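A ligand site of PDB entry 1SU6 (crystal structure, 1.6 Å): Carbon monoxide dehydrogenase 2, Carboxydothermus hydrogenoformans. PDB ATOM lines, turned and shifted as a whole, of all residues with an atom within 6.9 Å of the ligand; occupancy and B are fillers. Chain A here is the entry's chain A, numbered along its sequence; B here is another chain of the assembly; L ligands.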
ATOM      1  N   CYS A  47      22.817  20.892 -14.948  1.00  0.00           N
ATOM      2  CA  CYS A  47      21.984  20.099 -14.019  1.00  0.00           C
ATOM      3  C   CYS A  47      22.531  20.310 -12.623  1.00  0.00           C
ATOM      4  O   CYS A  47      23.770  20.352 -12.453  1.00  0.00           O
ATOM      5  CB  CYS A  47      21.950  18.608 -14.399  1.00  0.00           C
ATOM      6  SG  CYS A  47      21.108  17.611 -13.128  1.00  0.00           S
ATOM      7  N   CYS A  48      21.666  20.450 -11.621  1.00  0.00           N
ATOM      8  CA  CYS A  48      22.133  20.617 -10.249  1.00  0.00           C
ATOM      9  C   CYS A  48      21.306  19.745  -9.309  1.00  0.00           C
ATOM     10  O   CYS A  48      20.077  19.760  -9.373  1.00  0.00           O
ATOM     11  CB  CYS A  48      22.055  22.094  -9.797  1.00  0.00           C
ATOM     12  SG  CYS A  48      22.511  22.370  -8.068  1.00  0.00           S
ATOM     13  N   ARG A  49      22.010  19.005  -8.451  1.00  0.00           N
ATOM     14  CA  ARG A  49      21.359  18.189  -7.441  1.00  0.00           C
ATOM     15  C   ARG A  49      21.917  18.509  -6.052  1.00  0.00           C
ATOM     16  O   ARG A  49      21.963  17.585  -5.227  1.00  0.00           O
ATOM     17  CB  ARG A  49      21.532  16.689  -7.710  1.00  0.00           C
ATOM     18  CG  ARG A  49      20.933  16.225  -9.009  1.00  0.00           C
ATOM     19  CD  ARG A  49      21.395  14.809  -9.373  1.00  0.00           C
ATOM     20  NE  ARG A  49      21.164  13.870  -8.295  1.00  0.00           N
ATOM     21  CZ  ARG A  49      21.756  12.708  -8.059  1.00  0.00           C
ATOM     22  NH1 ARG A  49      22.696  12.223  -8.857  1.00  0.00           N
ATOM     23  NH2 ARG A  49      21.351  12.049  -6.972  1.00  0.00           N
ATOM     24  N   HIS A  50      22.297  19.756  -5.804  1.00  0.00           N
ATOM     25  CA  HIS A  50      22.926  20.143  -4.545  1.00  0.00           C
ATOM     26  C   HIS A  50      21.909  20.334  -3.403  1.00  0.00           C
ATOM     27  O   HIS A  50      22.380  20.630  -2.309  1.00  0.00           O
ATOM     28  CB  HIS A  50      23.756  21.410  -4.693  1.00  0.00           C
ATOM     29  CG  HIS A  50      24.969  21.209  -5.557  1.00  0.00           C
ATOM     30  ND1 HIS A  50      26.047  22.051  -5.526  1.00  0.00           N
ATOM     31  CD2 HIS A  50      25.255  20.243  -6.465  1.00  0.00           C
ATOM     32  CE1 HIS A  50      26.961  21.624  -6.382  1.00  0.00           C
ATOM     33  NE2 HIS A  50      26.516  20.522  -6.972  1.00  0.00           N
ATOM     34  N   CYS A  51      20.601  20.175  -3.649  1.00  0.00           N
ATOM     35  CA  CYS A  51      19.667  20.162  -2.528  1.00  0.00           C
ATOM     36  C   CYS A  51      18.459  19.321  -2.903  1.00  0.00           C
ATOM     37  O   CYS A  51      18.311  18.910  -4.049  1.00  0.00           O
ATOM     38  CB  CYS A  51      19.241  21.548  -2.064  1.00  0.00           C
ATOM     39  SG  CYS A  51      17.952  22.337  -3.065  1.00  0.00           S
ATOM     40  N   LEU A  52      17.620  19.033  -1.912  1.00  0.00           N
ATOM     41  CA  LEU A  52      16.517  18.117  -2.146  1.00  0.00           C
ATOM     42  C   LEU A  52      15.322  18.797  -2.800  1.00  0.00           C
ATOM     43  O   LEU A  52      14.257  18.180  -3.025  1.00  0.00           O
ATOM     44  CB  LEU A  52      16.133  17.441  -0.818  1.00  0.00           C
ATOM     45  CG  LEU A  52      17.244  16.671  -0.103  1.00  0.00           C
ATOM     46  CD1 LEU A  52      16.792  16.168   1.266  1.00  0.00           C
ATOM     47  CD2 LEU A  52      17.718  15.507  -0.952  1.00  0.00           C
ATOM     48  N   GLN A  53      15.456  20.085  -3.145  1.00  0.00           N
ATOM     49  CA  GLN A  53      14.406  20.647  -4.003  1.00  0.00           C
ATOM     50  C   GLN A  53      14.647  20.250  -5.454  1.00  0.00           C
ATOM     51  O   GLN A  53      13.789  20.381  -6.317  1.00  0.00           O
ATOM     52  CB  GLN A  53      14.341  22.173  -3.904  1.00  0.00           C
ATOM     53  CG  GLN A  53      14.047  22.616  -2.467  1.00  0.00           C
ATOM     54  CD  GLN A  53      14.033  24.134  -2.331  1.00  0.00           C
ATOM     55  OE1 GLN A  53      14.901  24.857  -2.820  1.00  0.00           O
ATOM     56  NE2 GLN A  53      13.014  24.604  -1.623  1.00  0.00           N
ATOM     57  N   GLY A  54      15.859  19.739  -5.673  1.00  0.00           N
ATOM     58  CA  GLY A  54      16.270  19.309  -6.986  1.00  0.00           C
ATOM     59  C   GLY A  54      15.684  17.957  -7.348  1.00  0.00           C
ATOM     60  O   GLY A  54      14.898  17.397  -6.578  1.00  0.00           O
ATOM     61  N   PRO A  55      16.042  17.403  -8.494  1.00  0.00           N
ATOM     62  CA  PRO A  55      17.031  18.001  -9.390  1.00  0.00           C
ATOM     63  C   PRO A  55      16.490  19.137 -10.245  1.00  0.00           C
ATOM     64  O   PRO A  55      15.349  19.176 -10.689  1.00  0.00           O
ATOM     65  CB  PRO A  55      17.407  16.847 -10.330  1.00  0.00           C
ATOM     66  CG  PRO A  55      16.489  15.710 -10.053  1.00  0.00           C
ATOM     67  CD  PRO A  55      15.531  16.093  -8.970  1.00  0.00           C
ATOM     68  N   CYS A  56      17.424  20.059 -10.445  1.00  0.00           N
ATOM     69  CA  CYS A  56      17.163  21.186 -11.319  1.00  0.00           C
ATOM     70  C   CYS A  56      17.936  21.033 -12.628  1.00  0.00           C
ATOM     71  O   CYS A  56      19.089  20.623 -12.682  1.00  0.00           O
ATOM     72  CB  CYS A  56      17.569  22.498 -10.638  1.00  0.00           C
ATOM     73  SG  CYS A  56      16.520  22.914  -9.229  1.00  0.00           S
ATOM     74  N   ARG A  57      17.287  21.420 -13.701  1.00  0.00           N
ATOM     75  CA  ARG A  57      18.018  21.419 -14.975  1.00  0.00           C
ATOM     76  C   ARG A  57      17.712  22.733 -15.675  1.00  0.00           C
ATOM     77  O   ARG A  57      16.760  23.436 -15.316  1.00  0.00           O
ATOM     78  CB  ARG A  57      17.621  20.190 -15.784  1.00  0.00           C
ATOM     79  CG  ARG A  57      16.241  20.356 -16.421  1.00  0.00           C
ATOM     80  CD  ARG A  57      15.602  18.998 -16.728  1.00  0.00           C
ATOM     81  NE  ARG A  57      14.264  19.254 -17.328  1.00  0.00           N
ATOM     82  CZ  ARG A  57      13.211  19.565 -16.549  1.00  0.00           C
ATOM     83  NH1 ARG A  57      12.075  19.762 -17.207  1.00  0.00           N
ATOM     84  NH2 ARG A  57      13.272  19.679 -15.204  1.00  0.00           N
ATOM     85  N   VAL A  67      16.283  28.720 -15.117  1.00  0.00           N
ATOM     86  CA  VAL A  67      16.937  29.005 -13.860  1.00  0.00           C
ATOM     87  C   VAL A  67      16.593  27.925 -12.838  1.00  0.00           C
ATOM     88  O   VAL A  67      15.526  27.322 -12.893  1.00  0.00           O
ATOM     89  CB  VAL A  67      16.564  30.426 -13.387  1.00  0.00           C
ATOM     90  CG1 VAL A  67      15.059  30.518 -13.151  1.00  0.00           C
ATOM     91  CG2 VAL A  67      17.330  30.840 -12.156  1.00  0.00           C
ATOM     92  N   GLY A  68      17.562  27.695 -11.961  1.00  0.00           N
ATOM     93  CA  GLY A  68      17.393  26.803 -10.813  1.00  0.00           C
ATOM     94  C   GLY A  68      16.271  27.238  -9.894  1.00  0.00           C
ATOM     95  O   GLY A  68      15.899  28.407  -9.821  1.00  0.00           O
ATOM     96  N   ILE A  69      15.696  26.289  -9.158  1.00  0.00           N
ATOM     97  CA  ILE A  69      14.604  26.630  -8.260  1.00  0.00           C
ATOM     98  C   ILE A  69      14.997  27.663  -7.217  1.00  0.00           C
ATOM     99  O   ILE A  69      14.189  28.556  -6.888  1.00  0.00           O
ATOM    100  CB  ILE A  69      14.077  25.337  -7.607  1.00  0.00           C
ATOM    101  CG1 ILE A  69      13.312  24.490  -8.609  1.00  0.00           C
ATOM    102  CG2 ILE A  69      13.250  25.653  -6.368  1.00  0.00           C
ATOM    103  CD1 ILE A  69      12.971  23.092  -8.132  1.00  0.00           C
ATOM    104  N   CYS A  70      16.198  27.628  -6.675  1.00  0.00           N
ATOM    105  CA  CYS A  70      16.618  28.624  -5.706  1.00  0.00           C
ATOM    106  C   CYS A  70      17.058  29.949  -6.338  1.00  0.00           C
ATOM    107  O   CYS A  70      17.448  30.833  -5.571  1.00  0.00           O
ATOM    108  CB  CYS A  70      17.804  28.056  -4.927  1.00  0.00           C
ATOM    109  SG  CYS A  70      19.205  27.682  -6.010  1.00  0.00           S
ATOM    110  N   GLY A  71      17.028  30.050  -7.663  1.00  0.00           N
ATOM    111  CA  GLY A  71      17.541  31.177  -8.407  1.00  0.00           C
ATOM    112  C   GLY A  71      18.917  30.989  -9.007  1.00  0.00           C
ATOM    113  O   GLY A  71      19.452  31.904  -9.638  1.00  0.00           O
ATOM    114  N   ALA A  72      19.564  29.845  -8.830  1.00  0.00           N
ATOM    115  CA  ALA A  72      20.902  29.603  -9.380  1.00  0.00           C
ATOM    116  C   ALA A  72      20.838  29.633 -10.898  1.00  0.00           C
ATOM    117  O   ALA A  72      20.071  28.928 -11.558  1.00  0.00           O
ATOM    118  CB  ALA A  72      21.483  28.278  -8.923  1.00  0.00           C
ATOM    119  N   THR A  73      21.713  30.490 -11.454  1.00  0.00           N
ATOM    120  CA  THR A  73      21.753  30.676 -12.898  1.00  0.00           C
ATOM    121  C   THR A  73      22.584  29.581 -13.560  1.00  0.00           C
ATOM    122  O   THR A  73      23.286  28.849 -12.874  1.00  0.00           O
ATOM    123  CB  THR A  73      22.390  32.028 -13.302  1.00  0.00           C
ATOM    124  OG1 THR A  73      23.697  32.066 -12.754  1.00  0.00           O
ATOM    125  CG2 THR A  73      21.621  33.224 -12.696  1.00  0.00           C
ATOM    126  N   ILE A  77      25.443  27.273 -11.743  1.00  0.00           N
ATOM    127  CA  ILE A  77      25.345  25.806 -11.707  1.00  0.00           C
ATOM    128  C   ILE A  77      26.574  25.205 -12.351  1.00  0.00           C
ATOM    129  O   ILE A  77      27.157  24.251 -11.824  1.00  0.00           O
ATOM    130  CB  ILE A  77      24.034  25.371 -12.402  1.00  0.00           C
ATOM    131  CG1 ILE A  77      22.846  25.781 -11.511  1.00  0.00           C
ATOM    132  CG2 ILE A  77      24.010  23.888 -12.709  1.00  0.00           C
ATOM    133  CD1 ILE A  77      21.497  25.487 -12.115  1.00  0.00           C
ATOM    134  N   ARG A  80      29.680  25.713 -10.172  1.00  0.00           N
ATOM    135  CA  ARG A  80      29.687  24.927  -8.923  1.00  0.00           C
ATOM    136  C   ARG A  80      30.031  23.478  -9.203  1.00  0.00           C
ATOM    137  O   ARG A  80      30.806  22.854  -8.487  1.00  0.00           O
ATOM    138  CB  ARG A  80      28.319  25.014  -8.221  1.00  0.00           C
ATOM    139  CG  ARG A  80      28.106  26.409  -7.615  1.00  0.00           C
ATOM    140  CD  ARG A  80      26.902  26.425  -6.674  1.00  0.00           C
ATOM    141  NE  ARG A  80      25.686  25.904  -7.301  1.00  0.00           N
ATOM    142  CZ  ARG A  80      24.447  26.120  -6.816  1.00  0.00           C
ATOM    143  NH1 ARG A  80      24.299  26.840  -5.704  1.00  0.00           N
ATOM    144  NH2 ARG A  80      23.384  25.624  -7.429  1.00  0.00           N
ATOM    145  N   THR A 197      29.948  25.714  -2.692  1.00  0.00           N
ATOM    146  CA  THR A 197      29.138  25.243  -3.779  1.00  0.00           C
ATOM    147  C   THR A 197      27.833  24.597  -3.301  1.00  0.00           C
ATOM    148  O   THR A 197      27.018  24.210  -4.145  1.00  0.00           O
ATOM    149  CB  THR A 197      29.863  24.193  -4.647  1.00  0.00           C
ATOM    150  OG1 THR A 197      30.304  23.132  -3.783  1.00  0.00           O
ATOM    151  CG2 THR A 197      31.087  24.816  -5.326  1.00  0.00           C
ATOM    152  N   SER A 198      27.665  24.517  -1.984  1.00  0.00           N
ATOM    153  CA  SER A 198      26.395  24.012  -1.457  1.00  0.00           C
ATOM    154  C   SER A 198      25.306  25.063  -1.616  1.00  0.00           C
ATOM    155  O   SER A 198      25.534  26.220  -2.025  1.00  0.00           O
ATOM    156  CB  SER A 198      26.588  23.551  -0.012  1.00  0.00           C
ATOM    157  OG  SER A 198      26.776  24.640   0.866  1.00  0.00           O
ATOM    158  N   MET A 199      24.065  24.667  -1.330  1.00  0.00           N
ATOM    159  CA  MET A 199      22.940  25.537  -1.697  1.00  0.00           C
ATOM    160  C   MET A 199      22.986  26.862  -0.947  1.00  0.00           C
ATOM    161  O   MET A 199      23.329  26.947   0.237  1.00  0.00           O
ATOM    162  CB  MET A 199      21.637  24.780  -1.409  1.00  0.00           C
ATOM    163  CG  MET A 199      20.391  25.577  -1.810  1.00  0.00           C
ATOM    164  SD  MET A 199      19.866  26.636  -0.457  1.00  0.00           S
ATOM    165  CE  MET A 199      18.209  27.067  -1.007  1.00  0.00           C
ATOM    166  N   GLY A 200      22.569  27.917  -1.648  1.00  0.00           N
ATOM    167  CA  GLY A 200      22.456  29.253  -1.113  1.00  0.00           C
ATOM    168  C   GLY A 200      23.737  29.836  -0.566  1.00  0.00           C
ATOM    169  O   GLY A 200      23.766  30.634   0.395  1.00  0.00           O
ATOM    170  N   VAL B  28      10.316  31.510  -5.867  1.00  0.00           N
ATOM    171  CA  VAL B  28      10.807  30.120  -5.735  1.00  0.00           C
ATOM    172  C   VAL B  28       9.712  29.143  -6.119  1.00  0.00           C
ATOM    173  O   VAL B  28       9.986  28.130  -6.774  1.00  0.00           O
ATOM    174  CB  VAL B  28      11.352  29.890  -4.307  1.00  0.00           C
ATOM    175  CG1 VAL B  28      10.258  30.035  -3.262  1.00  0.00           C
ATOM    176  CG2 VAL B  28      12.009  28.515  -4.187  1.00  0.00           C
ATOM    177  N   MET B  35      10.054  23.994 -13.361  1.00  0.00           N
ATOM    178  CA  MET B  35      10.974  22.859 -13.416  1.00  0.00           C
ATOM    179  C   MET B  35      10.248  21.528 -13.543  1.00  0.00           C
ATOM    180  O   MET B  35      10.880  20.476 -13.759  1.00  0.00           O
ATOM    181  CB  MET B  35      11.857  22.878 -12.154  1.00  0.00           C
ATOM    182  CG  MET B  35      13.080  21.978 -12.208  1.00  0.00           C
ATOM    183  SD  MET B  35      14.274  22.613 -13.403  1.00  0.00           S
ATOM    184  CE  MET B  35      14.750  24.171 -12.663  1.00  0.00           C
ATOM    185  N   GLN B  38      10.203  16.966 -12.859  1.00  0.00           N
ATOM    186  CA  GLN B  38      11.627  16.915 -12.550  1.00  0.00           C
ATOM    187  C   GLN B  38      12.207  15.567 -12.960  1.00  0.00           C
ATOM    188  O   GLN B  38      11.511  14.568 -13.123  1.00  0.00           O
ATOM    189  CB  GLN B  38      11.845  17.205 -11.059  1.00  0.00           C
ATOM    190  CG  GLN B  38      11.559  18.660 -10.695  1.00  0.00           C
ATOM    191  CD  GLN B  38      11.889  18.994  -9.255  1.00  0.00           C
ATOM    192  OE1 GLN B  38      12.997  19.456  -8.921  1.00  0.00           O
ATOM    193  NE2 GLN B  38      10.948  18.741  -8.371  1.00  0.00           N
ATOM    194  N   PRO B 336      19.881  32.772  -4.268  1.00  0.00           N
ATOM    195  CA  PRO B 336      20.532  33.843  -5.065  1.00  0.00           C
ATOM    196  C   PRO B 336      19.551  34.719  -5.820  1.00  0.00           C
ATOM    197  O   PRO B 336      19.958  35.799  -6.261  1.00  0.00           O
ATOM    198  CB  PRO B 336      21.436  33.095  -6.024  1.00  0.00           C
ATOM    199  CG  PRO B 336      20.808  31.722  -6.111  1.00  0.00           C
ATOM    200  CD  PRO B 336      20.337  31.439  -4.701  1.00  0.00           C
ATOM    201  N   MET B 560      15.777  20.056   3.099  1.00  0.00           N
ATOM    202  CA  MET B 560      16.217  20.599   1.819  1.00  0.00           C
ATOM    203  C   MET B 560      17.720  20.511   1.613  1.00  0.00           C
ATOM    204  O   MET B 560      18.242  19.905   0.673  1.00  0.00           O
ATOM    205  CB  MET B 560      15.761  22.078   1.717  1.00  0.00           C
ATOM    206  CG  MET B 560      16.144  22.741   0.394  1.00  0.00           C
ATOM    207  SD  MET B 560      17.688  23.674   0.411  1.00  0.00           S
ATOM    208  CE  MET B 560      17.349  24.855   1.723  1.00  0.00           C
HETATM  209 FE1  LIG L   1      19.296  25.370  -6.282  1.00  0.00          FE
HETATM  210 FE2  LIG L   1      20.656  23.138  -7.067  1.00  0.00          FE
HETATM  211 FE3  LIG L   1      17.984  23.329  -7.565  1.00  0.00          FE
HETATM  212 FE4  LIG L   1      18.852  22.985  -5.015  1.00  0.00          FE
HETATM  213  S1  LIG L   1      19.045  21.515  -6.730  1.00  0.00           S
HETATM  214  S2  LIG L   1      17.221  24.464  -5.791  1.00  0.00           S
HETATM  215  S3  LIG L   1      20.816  24.174  -5.118  1.00  0.00           S
HETATM  216  S4  LIG L   1      19.670  24.731  -8.469  1.00  0.00           S
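O of Cys 56 lies within hydrogen-bond range of N of Cys 48 (2.8 Å). The guanidinium group of Arg 80 sits close to the side-chain sulfur of Cys 48 (3.4 Å). SG of Cys 51 lies close to N of Gln 53 (3.4 Å). SG of Cys 51 sits close to SD of Met 560 of chain B (3.7 Å). The backbone NH (N) of Ile 69 lies close to the side-chain sulfur (SG) of Cys 56 (3.5 Å). The side-chain sulfur (SG) of Cys 70 sits close to the backbone NH (N) of Ala 72, 3.6 Å away. The side-chain amide oxygen (OE1) of Gln 38 of chain B sits close to the backbone carbonyl oxygen (O) of Gln 53 (2.9 Å). ND1 of His 50 lies within hydrogen-bond range of O of Thr 197 (2.7 Å).
His 50 touches the ligand. Gly 68 touches the ligand. Ile 69 touches the ligand. Met 199 touches the ligand. Hydrophobic or aromatic side chains that line the ligand: Ile 69 and Met 199. 11 residues have an atom within 4 Å of the ligand: Cys 48, His 50, Cys 51, Gln 53, Gly 54, Cys 56, Gly 68, Ile 69, Cys 70, Arg 80 and Met 199. The nearest printed residue that does not touch the ligand is Ala 72 (4.01 Å).
The side-chain sulfur (SG) of Cys 48 binds an iron atom (FE2) of the ligand, 2.2 Å away. N of Cys 51 lies close to S1 of the ligand, 3.7 Å away. An iron atom (FE4) of the ligand is bound by the side-chain sulfur of Cys 51, 2.2 Å away. SG of Cys 56 binds FE3 of the ligand (2.3 Å). The backbone NH of Cys 70 lies close to a sulfur (S2) of the ligand (3.4 Å). FE1 of the ligand is bound by SG of Cys 70, at 2.3 Å. S1 of the ligand sits close to N of Gly 54 (3.8 Å). The guanidinium group of Arg 80 lies close to a sulfur (S3) of the ligand (3.7 Å). S2 of the ligand sits close to OE1 of Gln 53, 3.8 Å away.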
